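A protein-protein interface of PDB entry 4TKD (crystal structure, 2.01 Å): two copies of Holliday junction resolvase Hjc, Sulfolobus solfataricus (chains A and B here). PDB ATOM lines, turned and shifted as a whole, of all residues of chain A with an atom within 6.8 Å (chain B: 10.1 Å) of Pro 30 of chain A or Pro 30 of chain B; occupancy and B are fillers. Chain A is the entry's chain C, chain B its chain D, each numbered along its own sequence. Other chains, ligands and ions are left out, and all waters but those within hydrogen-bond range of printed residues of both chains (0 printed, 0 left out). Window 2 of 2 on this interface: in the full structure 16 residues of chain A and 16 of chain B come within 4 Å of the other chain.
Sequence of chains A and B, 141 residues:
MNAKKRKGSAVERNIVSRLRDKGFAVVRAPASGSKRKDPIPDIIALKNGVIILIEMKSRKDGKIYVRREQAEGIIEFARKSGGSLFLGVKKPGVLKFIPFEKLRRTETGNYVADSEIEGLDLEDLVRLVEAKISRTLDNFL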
ATOM      1  N   VAL A  27       6.760  -5.403  24.324  1.00  0.00           N
ATOM      2  CA  VAL A  27       6.570  -4.043  24.785  1.00  0.00           C
ATOM      3  C   VAL A  27       6.778  -3.068  23.620  1.00  0.00           C
ATOM      4  O   VAL A  27       7.616  -3.304  22.753  1.00  0.00           O
ATOM      5  CB  VAL A  27       7.450  -3.728  26.044  1.00  0.00           C
ATOM      6  CG1 VAL A  27       8.929  -3.640  25.712  1.00  0.00           C
ATOM      7  CG2 VAL A  27       6.998  -2.469  26.746  1.00  0.00           C
ATOM      8  N   ARG A  28       6.019  -1.970  23.624  1.00  0.00           N
ATOM      9  CA  ARG A  28       6.137  -0.901  22.647  1.00  0.00           C
ATOM     10  C   ARG A  28       7.036   0.195  23.237  1.00  0.00           C
ATOM     11  O   ARG A  28       7.251   0.248  24.452  1.00  0.00           O
ATOM     12  CB  ARG A  28       4.756  -0.337  22.317  1.00  0.00           C
ATOM     13  CG  ARG A  28       3.947  -1.219  21.367  1.00  0.00           C
ATOM     14  CD  ARG A  28       2.483  -0.809  21.368  1.00  0.00           C
ATOM     15  NE  ARG A  28       2.051  -0.279  20.071  1.00  0.00           N
ATOM     16  CZ  ARG A  28       1.009  -0.734  19.377  1.00  0.00           C
ATOM     17  NH1 ARG A  28       0.272  -1.734  19.848  1.00  0.00           N
ATOM     18  NH2 ARG A  28       0.692  -0.187  18.211  1.00  0.00           N
ATOM     19  N   ALA A  29       7.570   1.067  22.402  1.00  0.00           N
ATOM     20  CA  ALA A  29       8.383   2.129  22.972  1.00  0.00           C
ATOM     21  C   ALA A  29       7.450   3.269  23.419  1.00  0.00           C
ATOM     22  O   ALA A  29       6.461   3.541  22.733  1.00  0.00           O
ATOM     23  CB  ALA A  29       9.383   2.632  21.958  1.00  0.00           C
ATOM     24  N   PRO A  30       7.722   3.938  24.563  1.00  0.00           N
ATOM     25  CA  PRO A  30       6.821   5.026  24.987  1.00  0.00           C
ATOM     26  C   PRO A  30       6.904   6.277  24.111  1.00  0.00           C
ATOM     27  O   PRO A  30       7.950   6.562  23.523  1.00  0.00           O
ATOM     28  CB  PRO A  30       7.237   5.306  26.439  1.00  0.00           C
ATOM     29  CG  PRO A  30       8.608   4.769  26.579  1.00  0.00           C
ATOM     30  CD  PRO A  30       8.823   3.714  25.534  1.00  0.00           C
ATOM     31  N   ALA A  31       5.784   7.030  24.031  1.00  0.00           N
ATOM     32  CA  ALA A  31       5.675   8.326  23.344  1.00  0.00           C
ATOM     33  C   ALA A  31       6.514   9.352  24.143  1.00  0.00           C
ATOM     34  O   ALA A  31       6.953  10.368  23.598  1.00  0.00           O
ATOM     35  CB  ALA A  31       4.217   8.763  23.285  1.00  0.00           C
ATOM     36  N   SER A  32       6.765   9.031  25.432  1.00  0.00           N
ATOM     37  CA  SER A  32       7.624   9.733  26.389  1.00  0.00           C
ATOM     38  C   SER A  32       9.102   9.233  26.206  1.00  0.00           C
ATOM     39  O   SER A  32       9.799   8.917  27.186  1.00  0.00           O
ATOM     40  CB  SER A  32       7.131   9.490  27.814  1.00  0.00           C
ATOM     41  OG  SER A  32       7.951  10.128  28.782  1.00  0.00           O
ATOM     42  N   GLY A  33       9.550   9.196  24.936  1.00  0.00           N
ATOM     43  CA  GLY A  33      10.889   8.751  24.559  1.00  0.00           C
ATOM     44  C   GLY A  33      11.266   8.995  23.110  1.00  0.00           C
ATOM     45  O   GLY A  33      10.837   9.992  22.508  1.00  0.00           O
ATOM     46  N   SER A  34      12.162   8.100  22.567  1.00  0.00           N
ATOM     47  CA  SER A  34      12.730   8.075  21.193  1.00  0.00           C
ATOM     48  C   SER A  34      13.202   9.452  20.653  1.00  0.00           C
ATOM     49  O   SER A  34      13.471   9.640  19.465  1.00  0.00           O
ATOM     50  CB  SER A  34      11.798   7.344  20.233  1.00  0.00           C
ATOM     51  OG  SER A  34      11.557   6.028  20.700  1.00  0.00           O
ATOM     52  N   ILE A  40      14.704   4.472  21.386  1.00  0.00           N
ATOM     53  CA  ILE A  40      14.355   3.126  21.813  1.00  0.00           C
ATOM     54  C   ILE A  40      13.640   2.471  20.651  1.00  0.00           C
ATOM     55  O   ILE A  40      12.729   3.085  20.081  1.00  0.00           O
ATOM     56  CB  ILE A  40      13.460   3.202  23.099  1.00  0.00           C
ATOM     57  CG1 ILE A  40      14.271   3.751  24.323  1.00  0.00           C
ATOM     58  CG2 ILE A  40      12.806   1.851  23.449  1.00  0.00           C
ATOM     59  CD1 ILE A  40      13.415   4.220  25.471  1.00  0.00           C
ATOM     60  N   PRO A  41      13.996   1.226  20.272  1.00  0.00           N
ATOM     61  CA  PRO A  41      13.222   0.539  19.203  1.00  0.00           C
ATOM     62  C   PRO A  41      11.708   0.490  19.493  1.00  0.00           C
ATOM     63  O   PRO A  41      11.303   0.362  20.657  1.00  0.00           O
ATOM     64  CB  PRO A  41      13.845  -0.862  19.170  1.00  0.00           C
ATOM     65  CG  PRO A  41      15.215  -0.680  19.774  1.00  0.00           C
ATOM     66  CD  PRO A  41      15.032   0.339  20.840  1.00  0.00           C
ATOM     67  N   ASP A  42      10.874   0.644  18.438  1.00  0.00           N
ATOM     68  CA  ASP A  42       9.399   0.653  18.495  1.00  0.00           C
ATOM     69  C   ASP A  42       8.826  -0.547  19.172  1.00  0.00           C
ATOM     70  O   ASP A  42       7.856  -0.412  19.916  1.00  0.00           O
ATOM     71  CB  ASP A  42       8.770   0.805  17.092  1.00  0.00           C
ATOM     72  CG  ASP A  42       9.078   2.145  16.461  1.00  0.00           C
ATOM     73  OD1 ASP A  42       8.935   3.175  17.153  1.00  0.00           O
ATOM     74  OD2 ASP A  42       9.463   2.165  15.278  1.00  0.00           O
ATOM     75  N   GLU B  12      13.490   6.269  39.857  1.00  0.00           N
ATOM     76  CA  GLU B  12      13.334   5.534  38.604  1.00  0.00           C
ATOM     77  C   GLU B  12      14.318   6.077  37.578  1.00  0.00           C
ATOM     78  O   GLU B  12      15.059   5.295  36.980  1.00  0.00           O
ATOM     79  CB  GLU B  12      11.874   5.633  38.106  1.00  0.00           C
ATOM     80  CG  GLU B  12      11.502   4.593  37.063  1.00  0.00           C
ATOM     81  CD  GLU B  12      10.019   4.440  36.770  1.00  0.00           C
ATOM     82  OE1 GLU B  12       9.686   3.799  35.748  1.00  0.00           O
ATOM     83  OE2 GLU B  12       9.190   4.927  37.572  1.00  0.00           O
ATOM     84  N   ARG B  13      14.382   7.420  37.446  1.00  0.00           N
ATOM     85  CA  ARG B  13      15.294   8.131  36.527  1.00  0.00           C
ATOM     86  C   ARG B  13      16.742   7.853  36.868  1.00  0.00           C
ATOM     87  O   ARG B  13      17.533   7.586  35.965  1.00  0.00           O
ATOM     88  CB  ARG B  13      14.985   9.648  36.467  1.00  0.00           C
ATOM     89  CG  ARG B  13      13.813   9.935  35.531  1.00  0.00           C
ATOM     90  CD  ARG B  13      13.459  11.401  35.400  1.00  0.00           C
ATOM     91  NE  ARG B  13      12.767  11.674  34.137  1.00  0.00           N
ATOM     92  CZ  ARG B  13      11.445  11.641  33.970  1.00  0.00           C
ATOM     93  NH1 ARG B  13      10.644  11.334  34.988  1.00  0.00           N
ATOM     94  NH2 ARG B  13      10.914  11.909  32.784  1.00  0.00           N
ATOM     95  N   VAL B  16      17.626   4.170  35.852  1.00  0.00           N
ATOM     96  CA  VAL B  16      17.787   4.139  34.400  1.00  0.00           C
ATOM     97  C   VAL B  16      19.175   4.708  34.003  1.00  0.00           C
ATOM     98  O   VAL B  16      19.905   4.076  33.246  1.00  0.00           O
ATOM     99  CB  VAL B  16      16.594   4.842  33.690  1.00  0.00           C
ATOM    100  CG1 VAL B  16      16.875   5.086  32.214  1.00  0.00           C
ATOM    101  CG2 VAL B  16      15.308   4.039  33.848  1.00  0.00           C
ATOM    102  N   ARG B  20      22.401   2.630  32.468  1.00  0.00           N
ATOM    103  CA  ARG B  20      22.969   3.116  31.205  1.00  0.00           C
ATOM    104  C   ARG B  20      24.480   3.362  31.322  1.00  0.00           C
ATOM    105  O   ARG B  20      25.232   2.927  30.434  1.00  0.00           O
ATOM    106  CB  ARG B  20      22.231   4.359  30.709  1.00  0.00           C
ATOM    107  CG  ARG B  20      20.912   3.987  30.041  1.00  0.00           C
ATOM    108  CD  ARG B  20      20.150   5.171  29.506  1.00  0.00           C
ATOM    109  NE  ARG B  20      18.917   4.718  28.869  1.00  0.00           N
ATOM    110  CZ  ARG B  20      17.797   5.428  28.824  1.00  0.00           C
ATOM    111  NH1 ARG B  20      17.755   6.644  29.351  1.00  0.00           N
ATOM    112  NH2 ARG B  20      16.709   4.926  28.253  1.00  0.00           N
ATOM    113  N   VAL B  26      18.313   0.391  28.111  1.00  0.00           N
ATOM    114  CA  VAL B  26      17.202   0.527  29.072  1.00  0.00           C
ATOM    115  C   VAL B  26      15.969   1.193  28.498  1.00  0.00           C
ATOM    116  O   VAL B  26      16.062   2.214  27.819  1.00  0.00           O
ATOM    117  CB  VAL B  26      17.654   1.267  30.386  1.00  0.00           C
ATOM    118  CG1 VAL B  26      16.633   1.084  31.514  1.00  0.00           C
ATOM    119  CG2 VAL B  26      19.022   0.798  30.860  1.00  0.00           C
ATOM    120  N   VAL B  27      14.806   0.631  28.828  1.00  0.00           N
ATOM    121  CA  VAL B  27      13.516   1.192  28.497  1.00  0.00           C
ATOM    122  C   VAL B  27      12.760   1.374  29.801  1.00  0.00           C
ATOM    123  O   VAL B  27      12.650   0.435  30.597  1.00  0.00           O
ATOM    124  CB  VAL B  27      12.704   0.475  27.367  1.00  0.00           C
ATOM    125  CG1 VAL B  27      12.401  -0.966  27.691  1.00  0.00           C
ATOM    126  CG2 VAL B  27      11.427   1.235  27.006  1.00  0.00           C
ATOM    127  N   ARG B  28      12.428   2.649  30.087  1.00  0.00           N
ATOM    128  CA  ARG B  28      11.626   3.107  31.221  1.00  0.00           C
ATOM    129  C   ARG B  28      10.212   3.072  30.634  1.00  0.00           C
ATOM    130  O   ARG B  28       9.708   4.075  30.137  1.00  0.00           O
ATOM    131  CB  ARG B  28      12.057   4.526  31.647  1.00  0.00           C
ATOM    132  CG  ARG B  28      11.622   4.913  33.050  1.00  0.00           C
ATOM    133  CD  ARG B  28      12.175   6.266  33.483  1.00  0.00           C
ATOM    134  NE  ARG B  28      11.470   7.371  32.828  1.00  0.00           N
ATOM    135  CZ  ARG B  28      10.445   8.038  33.354  1.00  0.00           C
ATOM    136  NH1 ARG B  28      10.009   7.747  34.576  1.00  0.00           N
ATOM    137  NH2 ARG B  28       9.856   9.008  32.667  1.00  0.00           N
ATOM    138  N   ALA B  29       9.664   1.843  30.568  1.00  0.00           N
ATOM    139  CA  ALA B  29       8.408   1.355  29.987  1.00  0.00           C
ATOM    140  C   ALA B  29       7.179   2.279  29.949  1.00  0.00           C
ATOM    141  O   ALA B  29       7.070   3.187  30.786  1.00  0.00           O
ATOM    142  CB  ALA B  29       8.044   0.026  30.623  1.00  0.00           C
ATOM    143  N   PRO B  30       6.211   2.024  29.013  1.00  0.00           N
ATOM    144  CA  PRO B  30       4.986   2.845  28.989  1.00  0.00           C
ATOM    145  C   PRO B  30       3.940   2.282  29.950  1.00  0.00           C
ATOM    146  O   PRO B  30       3.038   2.991  30.379  1.00  0.00           O
ATOM    147  CB  PRO B  30       4.516   2.745  27.529  1.00  0.00           C
ATOM    148  CG  PRO B  30       5.184   1.502  26.969  1.00  0.00           C
ATOM    149  CD  PRO B  30       6.166   0.974  27.969  1.00  0.00           C
ATOM    150  N   PRO B  39       0.458  -4.902  33.355  1.00  0.00           N
ATOM    151  CA  PRO B  39       1.309  -6.067  33.650  1.00  0.00           C
ATOM    152  C   PRO B  39       2.724  -6.002  33.033  1.00  0.00           C
ATOM    153  O   PRO B  39       3.331  -7.062  32.797  1.00  0.00           O
ATOM    154  CB  PRO B  39       0.480  -7.245  33.128  1.00  0.00           C
ATOM    155  CG  PRO B  39      -0.344  -6.667  32.021  1.00  0.00           C
ATOM    156  CD  PRO B  39      -0.614  -5.223  32.389  1.00  0.00           C
ATOM    157  N   ILE B  40       3.261  -4.760  32.789  1.00  0.00           N
ATOM    158  CA  ILE B  40       4.607  -4.536  32.237  1.00  0.00           C
ATOM    159  C   ILE B  40       5.527  -3.952  33.319  1.00  0.00           C
ATOM    160  O   ILE B  40       5.178  -2.917  33.900  1.00  0.00           O
ATOM    161  CB  ILE B  40       4.606  -3.663  30.938  1.00  0.00           C
ATOM    162  CG1 ILE B  40       3.813  -4.355  29.802  1.00  0.00           C
ATOM    163  CG2 ILE B  40       6.046  -3.311  30.467  1.00  0.00           C
ATOM    164  CD1 ILE B  40       3.423  -3.434  28.606  1.00  0.00           C
ATOM    165  N   PRO B  41       6.714  -4.566  33.578  1.00  0.00           N
ATOM    166  CA  PRO B  41       7.646  -3.978  34.547  1.00  0.00           C
ATOM    167  C   PRO B  41       8.034  -2.533  34.191  1.00  0.00           C
ATOM    168  O   PRO B  41       8.153  -2.195  33.008  1.00  0.00           O
ATOM    169  CB  PRO B  41       8.851  -4.921  34.490  1.00  0.00           C
ATOM    170  CG  PRO B  41       8.304  -6.194  33.966  1.00  0.00           C
ATOM    171  CD  PRO B  41       7.294  -5.774  32.969  1.00  0.00           C
ATOM    172  N   ASP B  42       8.202  -1.682  35.224  1.00  0.00           N
ATOM    173  CA  ASP B  42       8.539  -0.262  35.102  1.00  0.00           C
ATOM    174  C   ASP B  42       9.798  -0.019  34.301  1.00  0.00           C
ATOM    175  O   ASP B  42       9.866   0.935  33.525  1.00  0.00           O
ATOM    176  CB  ASP B  42       8.634   0.411  36.485  1.00  0.00           C
ATOM    177  CG  ASP B  42       7.306   0.443  37.228  1.00  0.00           C
ATOM    178  OD1 ASP B  42       6.279   0.792  36.601  1.00  0.00           O
ATOM    179  OD2 ASP B  42       7.295   0.127  38.433  1.00  0.00           O
ATOM    180  N   ILE B  43      10.799  -0.878  34.505  1.00  0.00           N
ATOM    181  CA  ILE B  43      12.094  -0.764  33.848  1.00  0.00           C
ATOM    182  C   ILE B  43      12.490  -2.115  33.295  1.00  0.00           C
ATOM    183  O   ILE B  43      12.431  -3.135  34.001  1.00  0.00           O
ATOM    184  CB  ILE B  43      13.187  -0.230  34.830  1.00  0.00           C
ATOM    185  CG1 ILE B  43      12.820   1.132  35.445  1.00  0.00           C
ATOM    186  CG2 ILE B  43      14.573  -0.200  34.179  1.00  0.00           C
ATOM    187  CD1 ILE B  43      13.649   1.516  36.710  1.00  0.00           C
ATOM    188  N   ILE B  44      12.920  -2.107  32.037  1.00  0.00           N
ATOM    189  CA  ILE B  44      13.468  -3.262  31.360  1.00  0.00           C
ATOM    190  C   ILE B  44      14.891  -2.862  30.958  1.00  0.00           C
ATOM    191  O   ILE B  44      15.069  -1.866  30.240  1.00  0.00           O
ATOM    192  CB  ILE B  44      12.610  -3.711  30.166  1.00  0.00           C
ATOM    193  CG1 ILE B  44      11.195  -4.157  30.646  1.00  0.00           C
ATOM    194  CG2 ILE B  44      13.343  -4.809  29.390  1.00  0.00           C
ATOM    195  CD1 ILE B  44      10.082  -4.026  29.646  1.00  0.00           C
ATOM    196  N   GLU B  55      10.395  -3.436  39.055  1.00  0.00           N
ATOM    197  CA  GLU B  55       9.113  -2.868  39.405  1.00  0.00           C
ATOM    198  C   GLU B  55       9.351  -1.903  40.563  1.00  0.00           C
ATOM    199  O   GLU B  55       9.903  -2.294  41.587  1.00  0.00           O
ATOM    200  CB  GLU B  55       8.105  -3.975  39.769  1.00  0.00           C
ATOM    201  CG  GLU B  55       6.671  -3.481  39.893  1.00  0.00           C
ATOM    202  CD  GLU B  55       5.953  -3.039  38.636  1.00  0.00           C
ATOM    203  OE1 GLU B  55       6.562  -3.033  37.541  1.00  0.00           O
ATOM    204  OE2 GLU B  55       4.760  -2.690  38.755  1.00  0.00           O
ATOM    205  N   PHE B  77       5.415 -11.818  32.868  1.00  0.00           N
ATOM    206  CA  PHE B  77       6.312 -11.126  31.951  1.00  0.00           C
ATOM    207  C   PHE B  77       7.732 -11.675  32.152  1.00  0.00           C
ATOM    208  O   PHE B  77       8.372 -12.031  31.174  1.00  0.00           O
ATOM    209  CB  PHE B  77       6.253  -9.615  32.192  1.00  0.00           C
ATOM    210  CG  PHE B  77       6.874  -8.775  31.101  1.00  0.00           C
ATOM    211  CD1 PHE B  77       8.243  -8.530  31.084  1.00  0.00           C
ATOM    212  CD2 PHE B  77       6.083  -8.185  30.119  1.00  0.00           C
ATOM    213  CE1 PHE B  77       8.811  -7.702  30.110  1.00  0.00           C
ATOM    214  CE2 PHE B  77       6.650  -7.353  29.148  1.00  0.00           C
ATOM    215  CZ  PHE B  77       8.012  -7.115  29.152  1.00  0.00           C
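Pro 30 of chain B touches Val 27 of chain A. CG2 of Ile 40 of chain B touches CG2 of Val 27 of chain A (3.9 Å). O of Arg 28 of chain A touches CG of Pro 30 of chain B, 3.5 Å away. CD of Pro 30 of chain A touches CG2 of Val 27 of chain B, at 3.9 Å. Pro 30 of chain A touches Arg 28 of chain B (CG to O, 3.8 Å). Pro 30 of chain B touches Pro 30 of chain A (CB to CB, 3.9 Å). Ile 40 of chain A touches Val 27 of chain B (CG2 to CG2, 3.9 Å).
Val 27 of chain A touches Pro 30 of chain B, and with the chains exchanged Pro 30 of chain A touches Val 27 of chain B. Val 27 of chain A touches Ile 40 of chain B, and with the chains exchanged Ile 40 of chain A touches Val 27 of chain B. Arg 28 of chain A touches Pro 30 of chain B, and with the chains exchanged Pro 30 of chain A touches Arg 28 of chain B. Pro 30 of chain A touches its own counterpart, Pro 30 of chain B.
Ala 29 of chain A touches none of the printed residues of chain B. Printed residues of chain B within 4 Å of Pro 30 of chain A: Val 27, Arg 28 and Pro 30. No residue of chain B comes within 4 Å of Ala 31 of chain A. Ser 32 of chain A touches none of the printed residues of chain B. Of the printed residues of chain B, Ile 40 of chain A touches Val 27 (3.9 Å). Printed residues of chain A within 4 Å of Arg 28 of chain B: Pro 30. Printed residues of chain A within 4 Å of Pro 30 of chain B: Val 27, Arg 28 and Pro 30. Printed residues of chain A within 4 Å of Ile 40 of chain B: Val 27. Pro 41 of chain B touches none of the printed residues of chain A. Ile 43 of chain B touches none of the printed residues of chain A. The nearest residue of chain B that does not touch Pro 30 of chain A is Ala 29 of chain B (4.4 Å). The nearest residue of chain A that does not touch Pro 30 of chain B is Ala 29 of chain A (4.6 Å). The nearest printed residue of chain B that does not touch Ile 40 of chain A is Val 26 of chain B (4.1 Å).
Hydrophobic or aromatic side chains of chain A within 4 Å of the printed part of chain B: Val 27, Pro 30 and Ile 40. Along chain A the printed residues that touch a printed residue of chain B span positions 27 to 40. Of the 17 printed residues of chain B, 4 touch a printed residue of chain A. Printed residues of chain B that touch a printed residue of chain A: Val 27, Arg 28, Pro 30 and Ile 40. Among the printed residues, 7 pairs touch across the chains.
O of Ile 40 of chain A is in hydrogen-bond range of OG of Ser 34 of chain A, 3.2 Å away. The backbone carbonyl oxygen (O) of Ile 44 of chain B sits at hydrogen-bond distance from the backbone NH (N) of Val 27 of chain B (2.9 Å).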
